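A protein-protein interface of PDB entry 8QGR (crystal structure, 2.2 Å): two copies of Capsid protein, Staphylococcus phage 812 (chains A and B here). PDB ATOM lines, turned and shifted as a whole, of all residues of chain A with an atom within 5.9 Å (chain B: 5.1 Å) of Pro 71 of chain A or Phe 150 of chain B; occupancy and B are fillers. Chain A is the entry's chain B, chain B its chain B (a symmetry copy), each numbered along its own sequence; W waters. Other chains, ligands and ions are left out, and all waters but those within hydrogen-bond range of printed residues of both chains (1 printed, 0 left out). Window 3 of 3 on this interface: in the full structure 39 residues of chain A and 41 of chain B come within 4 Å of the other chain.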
ATOM      1  N   CYS A  68     -20.328 -11.085 -11.653  1.00  0.00           N
ATOM      2  CA  CYS A  68     -21.312 -10.509 -12.557  1.00  0.00           C
ATOM      3  C   CYS A  68     -20.696  -9.360 -13.348  1.00  0.00           C
ATOM      4  O   CYS A  68     -21.316  -8.837 -14.269  1.00  0.00           O
ATOM      5  CB  CYS A  68     -22.521  -9.957 -11.811  1.00  0.00           C
ATOM      6  SG  CYS A  68     -22.119  -8.570 -10.708  1.00  0.00           S
ATOM      7  N   LEU A  69     -19.467  -8.988 -12.993  1.00  0.00           N
ATOM      8  CA  LEU A  69     -18.811  -7.832 -13.570  1.00  0.00           C
ATOM      9  C   LEU A  69     -18.994  -7.796 -15.083  1.00  0.00           C
ATOM     10  O   LEU A  69     -18.920  -8.828 -15.749  1.00  0.00           O
ATOM     11  CB  LEU A  69     -17.317  -7.892 -13.260  1.00  0.00           C
ATOM     12  CG  LEU A  69     -16.921  -7.906 -11.789  1.00  0.00           C
ATOM     13  CD1 LEU A  69     -15.435  -7.607 -11.663  1.00  0.00           C
ATOM     14  CD2 LEU A  69     -17.751  -6.919 -10.977  1.00  0.00           C
ATOM     15  N   ASN A  70     -19.169  -6.575 -15.604  1.00  0.00           N
ATOM     16  CA  ASN A  70     -19.182  -6.328 -17.034  1.00  0.00           C
ATOM     17  C   ASN A  70     -17.738  -6.296 -17.526  1.00  0.00           C
ATOM     18  O   ASN A  70     -16.951  -5.460 -17.092  1.00  0.00           O
ATOM     19  CB  ASN A  70     -19.947  -5.042 -17.362  1.00  0.00           C
ATOM     20  CG  ASN A  70     -19.987  -4.729 -18.841  1.00  0.00           C
ATOM     21  OD1 ASN A  70     -19.143  -5.181 -19.612  1.00  0.00           O
ATOM     22  ND2 ASN A  70     -20.946  -3.914 -19.240  1.00  0.00           N
ATOM     23  N   PRO A  71     -17.342  -7.222 -18.429  1.00  0.00           N
ATOM     24  CA  PRO A  71     -15.953  -7.331 -18.873  1.00  0.00           C
ATOM     25  C   PRO A  71     -15.436  -6.044 -19.496  1.00  0.00           C
ATOM     26  O   PRO A  71     -14.246  -5.775 -19.467  1.00  0.00           O
ATOM     27  CB  PRO A  71     -15.978  -8.456 -19.918  1.00  0.00           C
ATOM     28  CG  PRO A  71     -17.218  -9.250 -19.576  1.00  0.00           C
ATOM     29  CD  PRO A  71     -18.207  -8.232 -19.051  1.00  0.00           C
ATOM     30  N   ASP A  72     -16.358  -5.248 -20.030  1.00  0.00           N
ATOM     31  CA  ASP A  72     -16.023  -4.024 -20.733  1.00  0.00           C
ATOM     32  C   ASP A  72     -15.698  -2.896 -19.752  1.00  0.00           C
ATOM     33  O   ASP A  72     -14.845  -2.064 -20.042  1.00  0.00           O
ATOM     34  CB  ASP A  72     -17.164  -3.650 -21.684  1.00  0.00           C
ATOM     35  CG  ASP A  72     -17.357  -4.651 -22.816  1.00  0.00           C
ATOM     36  OD1 ASP A  72     -16.446  -5.483 -23.029  1.00  0.00           O
ATOM     37  OD2 ASP A  72     -18.426  -4.614 -23.451  1.00  0.00           O
ATOM     38  N   THR A  73     -16.363  -2.861 -18.591  1.00  0.00           N
ATOM     39  CA  THR A  73     -16.233  -1.714 -17.705  1.00  0.00           C
ATOM     40  C   THR A  73     -15.578  -2.083 -16.376  1.00  0.00           C
ATOM     41  O   THR A  73     -14.944  -1.243 -15.754  1.00  0.00           O
ATOM     42  CB  THR A  73     -17.601  -1.067 -17.458  1.00  0.00           C
ATOM     43  OG1 THR A  73     -18.431  -2.041 -16.834  1.00  0.00           O
ATOM     44  CG2 THR A  73     -18.266  -0.583 -18.726  1.00  0.00           C
ATOM     45  N   GLY A  74     -15.759  -3.323 -15.925  1.00  0.00           N
ATOM     46  CA  GLY A  74     -15.265  -3.731 -14.618  1.00  0.00           C
ATOM     47  C   GLY A  74     -16.275  -3.448 -13.504  1.00  0.00           C
ATOM     48  O   GLY A  74     -15.982  -3.676 -12.329  1.00  0.00           O
ATOM     49  N   ARG A  77     -23.131  -5.689 -12.099  1.00  0.00           N
ATOM     50  CA  ARG A  77     -24.434  -5.443 -12.676  1.00  0.00           C
ATOM     51  C   ARG A  77     -25.273  -4.726 -11.624  1.00  0.00           C
ATOM     52  O   ARG A  77     -25.348  -5.162 -10.481  1.00  0.00           O
ATOM     53  CB  ARG A  77     -25.118  -6.749 -13.090  1.00  0.00           C
ATOM     54  CG  ARG A  77     -24.275  -7.641 -13.983  1.00  0.00           C
ATOM     55  CD  ARG A  77     -23.916  -6.974 -15.295  1.00  0.00           C
ATOM     56  NE  ARG A  77     -22.954  -7.760 -16.059  1.00  0.00           N
ATOM     57  CZ  ARG A  77     -22.591  -7.493 -17.310  1.00  0.00           C
ATOM     58  NH1 ARG A  77     -21.742  -8.286 -17.941  1.00  0.00           N
ATOM     59  NH2 ARG A  77     -23.105  -6.448 -17.937  1.00  0.00           N
ATOM     60  N   ILE B 148     -10.300 -12.299  -8.600  1.00  0.00           N
ATOM     61  CA  ILE B 148     -11.259 -12.419  -9.689  1.00  0.00           C
ATOM     62  C   ILE B 148     -10.601 -11.998 -11.000  1.00  0.00           C
ATOM     63  O   ILE B 148      -9.860 -11.022 -11.039  1.00  0.00           O
ATOM     64  CB  ILE B 148     -12.523 -11.595  -9.384  1.00  0.00           C
ATOM     65  CG1 ILE B 148     -13.568 -11.716 -10.496  1.00  0.00           C
ATOM     66  CG2 ILE B 148     -12.162 -10.143  -9.133  1.00  0.00           C
ATOM     67  CD1 ILE B 148     -14.913 -11.116 -10.141  1.00  0.00           C
ATOM     68  N   TYR B 149     -10.943 -12.695 -12.084  1.00  0.00           N
ATOM     69  CA  TYR B 149     -10.250 -12.516 -13.346  1.00  0.00           C
ATOM     70  C   TYR B 149     -11.178 -12.728 -14.535  1.00  0.00           C
ATOM     71  O   TYR B 149     -12.046 -13.595 -14.504  1.00  0.00           O
ATOM     72  CB  TYR B 149      -9.158 -13.577 -13.495  1.00  0.00           C
ATOM     73  CG  TYR B 149      -8.216 -13.726 -12.332  1.00  0.00           C
ATOM     74  CD1 TYR B 149      -7.165 -12.842 -12.139  1.00  0.00           C
ATOM     75  CD2 TYR B 149      -8.383 -14.749 -11.411  1.00  0.00           C
ATOM     76  CE1 TYR B 149      -6.281 -12.996 -11.084  1.00  0.00           C
ATOM     77  CE2 TYR B 149      -7.518 -14.908 -10.341  1.00  0.00           C
ATOM     78  CZ  TYR B 149      -6.464 -14.025 -10.177  1.00  0.00           C
ATOM     79  OH  TYR B 149      -5.591 -14.166  -9.125  1.00  0.00           O
ATOM     80  N   PHE B 150     -10.929 -11.970 -15.607  1.00  0.00           N
ATOM     81  CA  PHE B 150     -11.555 -12.240 -16.887  1.00  0.00           C
ATOM     82  C   PHE B 150     -10.689 -13.244 -17.647  1.00  0.00           C
ATOM     83  O   PHE B 150      -9.516 -12.994 -17.901  1.00  0.00           O
ATOM     84  CB  PHE B 150     -11.754 -10.971 -17.719  1.00  0.00           C
ATOM     85  CG  PHE B 150     -12.549 -11.238 -18.972  1.00  0.00           C
ATOM     86  CD1 PHE B 150     -13.901 -11.541 -18.892  1.00  0.00           C
ATOM     87  CD2 PHE B 150     -11.930 -11.304 -20.213  1.00  0.00           C
ATOM     88  CE1 PHE B 150     -14.631 -11.844 -20.031  1.00  0.00           C
ATOM     89  CE2 PHE B 150     -12.667 -11.589 -21.354  1.00  0.00           C
ATOM     90  CZ  PHE B 150     -14.011 -11.865 -21.259  1.00  0.00           C
ATOM     91  N   VAL B 151     -11.278 -14.379 -18.019  1.00  0.00           N
ATOM     92  CA  VAL B 151     -10.520 -15.495 -18.566  1.00  0.00           C
ATOM     93  C   VAL B 151     -10.434 -15.394 -20.088  1.00  0.00           C
ATOM     94  O   VAL B 151     -11.370 -15.755 -20.792  1.00  0.00           O
ATOM     95  CB  VAL B 151     -11.165 -16.825 -18.133  1.00  0.00           C
ATOM     96  CG1 VAL B 151     -10.399 -18.034 -18.653  1.00  0.00           C
ATOM     97  CG2 VAL B 151     -11.311 -16.892 -16.627  1.00  0.00           C
ATOM     98  N   ASN B 152      -9.294 -14.924 -20.596  1.00  0.00           N
ATOM     99  CA  ASN B 152      -9.075 -14.841 -22.033  1.00  0.00           C
ATOM    100  C   ASN B 152      -8.359 -16.112 -22.491  1.00  0.00           C
ATOM    101  O   ASN B 152      -8.102 -17.010 -21.696  1.00  0.00           O
ATOM    102  CB  ASN B 152      -8.314 -13.570 -22.410  1.00  0.00           C
ATOM    103  CG  ASN B 152      -6.987 -13.466 -21.692  1.00  0.00           C
ATOM    104  OD1 ASN B 152      -6.263 -14.451 -21.590  1.00  0.00           O
ATOM    105  ND2 ASN B 152      -6.694 -12.307 -21.126  1.00  0.00           N
ATOM    106  N   ARG B 155      -5.026 -16.828 -20.771  1.00  0.00           N
ATOM    107  CA  ARG B 155      -5.170 -17.342 -19.418  1.00  0.00           C
ATOM    108  C   ARG B 155      -5.557 -18.824 -19.423  1.00  0.00           C
ATOM    109  O   ARG B 155      -5.173 -19.561 -18.517  1.00  0.00           O
ATOM    110  CB  ARG B 155      -6.138 -16.451 -18.631  1.00  0.00           C
ATOM    111  CG  ARG B 155      -5.500 -15.139 -18.202  1.00  0.00           C
ATOM    112  CD  ARG B 155      -6.409 -14.153 -17.488  1.00  0.00           C
ATOM    113  NE  ARG B 155      -5.593 -13.082 -16.927  1.00  0.00           N
ATOM    114  CZ  ARG B 155      -6.053 -11.955 -16.389  1.00  0.00           C
ATOM    115  NH1 ARG B 155      -5.208 -11.082 -15.869  1.00  0.00           N
ATOM    116  NH2 ARG B 155      -7.351 -11.711 -16.358  1.00  0.00           N
ATOM    117  N   ASN B 199     -13.683 -16.319 -21.933  1.00  0.00           N
ATOM    118  CA  ASN B 199     -14.604 -15.194 -21.993  1.00  0.00           C
ATOM    119  C   ASN B 199     -15.612 -15.243 -20.846  1.00  0.00           C
ATOM    120  O   ASN B 199     -16.647 -14.599 -20.905  1.00  0.00           O
ATOM    121  CB  ASN B 199     -15.250 -15.081 -23.375  1.00  0.00           C
ATOM    122  CG  ASN B 199     -14.264 -14.602 -24.426  1.00  0.00           C
ATOM    123  OD1 ASN B 199     -13.202 -14.059 -24.112  1.00  0.00           O
ATOM    124  ND2 ASN B 199     -14.617 -14.777 -25.687  1.00  0.00           N
ATOM    125  N   HIS B 200     -15.300 -15.997 -19.792  1.00  0.00           N
ATOM    126  CA  HIS B 200     -16.058 -15.910 -18.558  1.00  0.00           C
ATOM    127  C   HIS B 200     -15.222 -15.151 -17.536  1.00  0.00           C
ATOM    128  O   HIS B 200     -14.027 -14.950 -17.739  1.00  0.00           O
ATOM    129  CB  HIS B 200     -16.375 -17.291 -17.975  1.00  0.00           C
ATOM    130  CG  HIS B 200     -17.332 -18.096 -18.780  1.00  0.00           C
ATOM    131  ND1 HIS B 200     -17.157 -18.334 -20.125  1.00  0.00           N
ATOM    132  CD2 HIS B 200     -18.475 -18.693 -18.437  1.00  0.00           C
ATOM    133  CE1 HIS B 200     -18.171 -19.066 -20.563  1.00  0.00           C
ATOM    134  NE2 HIS B 200     -18.976 -19.304 -19.551  1.00  0.00           N
ATOM    135  N   THR B 201     -15.892 -14.734 -16.454  1.00  0.00           N
ATOM    136  CA  THR B 201     -15.250 -14.199 -15.266  1.00  0.00           C
ATOM    137  C   THR B 201     -15.227 -15.298 -14.208  1.00  0.00           C
ATOM    138  O   THR B 201     -16.267 -15.883 -13.886  1.00  0.00           O
ATOM    139  CB  THR B 201     -16.005 -12.977 -14.726  1.00  0.00           C
ATOM    140  OG1 THR B 201     -15.907 -11.886 -15.638  1.00  0.00           O
ATOM    141  CG2 THR B 201     -15.490 -12.509 -13.385  1.00  0.00           C
ATOM    142  N   TYR B 256      -7.913  -7.690 -13.551  1.00  0.00           N
ATOM    143  CA  TYR B 256      -9.174  -8.298 -13.926  1.00  0.00           C
ATOM    144  C   TYR B 256      -9.164  -8.572 -15.424  1.00  0.00           C
ATOM    145  O   TYR B 256      -9.439  -9.694 -15.833  1.00  0.00           O
ATOM    146  CB  TYR B 256     -10.373  -7.420 -13.550  1.00  0.00           C
ATOM    147  CG  TYR B 256     -11.682  -7.898 -14.132  1.00  0.00           C
ATOM    148  CD1 TYR B 256     -12.205  -9.140 -13.805  1.00  0.00           C
ATOM    149  CD2 TYR B 256     -12.370  -7.138 -15.065  1.00  0.00           C
ATOM    150  CE1 TYR B 256     -13.385  -9.596 -14.365  1.00  0.00           C
ATOM    151  CE2 TYR B 256     -13.560  -7.577 -15.626  1.00  0.00           C
ATOM    152  CZ  TYR B 256     -14.069  -8.812 -15.275  1.00  0.00           C
ATOM    153  OH  TYR B 256     -15.243  -9.255 -15.840  1.00  0.00           O
ATOM    154  N   LYS B 257      -8.855  -7.535 -16.217  1.00  0.00           N
ATOM    155  CA  LYS B 257      -8.800  -7.664 -17.666  1.00  0.00           C
ATOM    156  C   LYS B 257      -7.620  -6.886 -18.247  1.00  0.00           C
ATOM    157  O   LYS B 257      -7.322  -5.773 -17.824  1.00  0.00           O
ATOM    158  CB  LYS B 257     -10.103  -7.177 -18.305  1.00  0.00           C
ATOM    159  CG  LYS B 257     -10.149  -7.365 -19.812  1.00  0.00           C
ATOM    160  CD  LYS B 257     -11.529  -7.237 -20.392  1.00  0.00           C
ATOM    161  CE  LYS B 257     -11.546  -7.517 -21.877  1.00  0.00           C
ATOM    162  NZ  LYS B 257     -12.930  -7.525 -22.399  1.00  0.00           N
ATOM    163  N   LEU B 266      -7.508  -3.143 -16.908  1.00  0.00           N
ATOM    164  CA  LEU B 266      -8.743  -2.811 -16.225  1.00  0.00           C
ATOM    165  C   LEU B 266      -8.849  -3.574 -14.908  1.00  0.00           C
ATOM    166  O   LEU B 266      -8.813  -4.806 -14.882  1.00  0.00           O
ATOM    167  CB  LEU B 266      -9.910  -3.152 -17.150  1.00  0.00           C
ATOM    168  CG  LEU B 266     -11.291  -2.899 -16.557  1.00  0.00           C
ATOM    169  CD1 LEU B 266     -11.445  -1.435 -16.193  1.00  0.00           C
ATOM    170  CD2 LEU B 266     -12.384  -3.335 -17.523  1.00  0.00           C
HETATM  171  O   HOH W   1     -19.340 -11.394 -15.617  1.00  0.00           O
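Asn 70 of chain A touches none of the printed residues of chain B.
Pro 71 of chain A touches four residues of chain B.
Phe 150 of chain B touches just one residue of chain A: Pro 71.
Val 151 of chain B touches none of the printed residues of chain A.
Printed residues of chain A within 4 Å of Tyr 256 of chain B: Leu 69 and Pro 71.
Of the printed residues of chain A, Leu 266 of chain B touches Pro 71 (3.6 Å), Asp 72 (3.7 Å), Thr 73 (3.5 Å) and Gly 74 (3.7 Å).
The nearest printed residue of chain B that does not touch Thr 73 of chain A is Tyr 256 of chain B (5.9 Å).
The backbone NH (N) of Tyr 256 of chain B sits at hydrogen-bond distance from the backbone carbonyl oxygen (O) of Leu 266 of chain B (3.3 Å).
The side-chain hydroxyl (OH) of Tyr 256 of chain B sits at hydrogen-bond distance from the side-chain hydroxyl (OG1) of Thr 201 of chain B, at 2.7 Å.
The guanidinium group of Arg 155 of chain B sits at hydrogen-bond distance from the backbone carbonyl oxygen of Tyr 256 of chain B, at 3.0 Å.
NH2 of Arg 155 of chain B is in hydrogen-bond range of O of Phe 150 of chain B, 3.0 Å away.
N of Asp 72 of chain A is in hydrogen-bond range of OD1 of Asn 70 of chain A, at 2.8 Å.
O of Lys 257 of chain B sits at hydrogen-bond distance from N of Leu 266 of chain B.
Water W1 bridges O of Leu 69 of chain A and OG1 of Thr 201 of chain B.
Leu 69 of chain A touches Ile 148 of chain B.
Tyr 256 of chain B touches Leu 69 of chain A.
CB of Pro 71 of chain A touches CE1 of Phe 150 of chain B, 3.6 Å away.
Pro 71 of chain A touches Tyr 256 of chain B (CA to OH, 3.7 Å).
Lys 257 of chain B touches Pro 71 of chain A.
CD2 of Leu 266 of chain B touches O of Pro 71 of chain A (3.6 Å).
Leu 266 of chain B touches Asp 72 of chain A (CD2 to O, 3.7 Å).
O of Thr 73 of chain A touches CD1 of Leu 266 of chain B, 3.5 Å away.
Gly 74 of chain A touches Leu 266 of chain B (N to CD2, 3.7 Å).
Printed residues of chain A that touch a printed residue of chain B: Leu 69, Pro 71, Asp 72, Thr 73 and Gly 74.
Hydrophobic or aromatic side chains of chain A within 4 Å of the printed part of chain B: Leu 69 and Pro 71.
Along chain A the printed residues that touch a printed residue of chain B span positions 69 to 74.
Hydrophobic or aromatic side chains of chain B within 4 Å of the printed part of chain A: Ile 148, Phe 150, Tyr 256 and Leu 266.
Among the printed residues, 9 pairs touch across the chains.
Among the printed residues, no Asp or Glu carboxylate lies within 4 Å of a Lys or Arg side-chain nitrogen of the other chain.
No position is printed for both chains.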
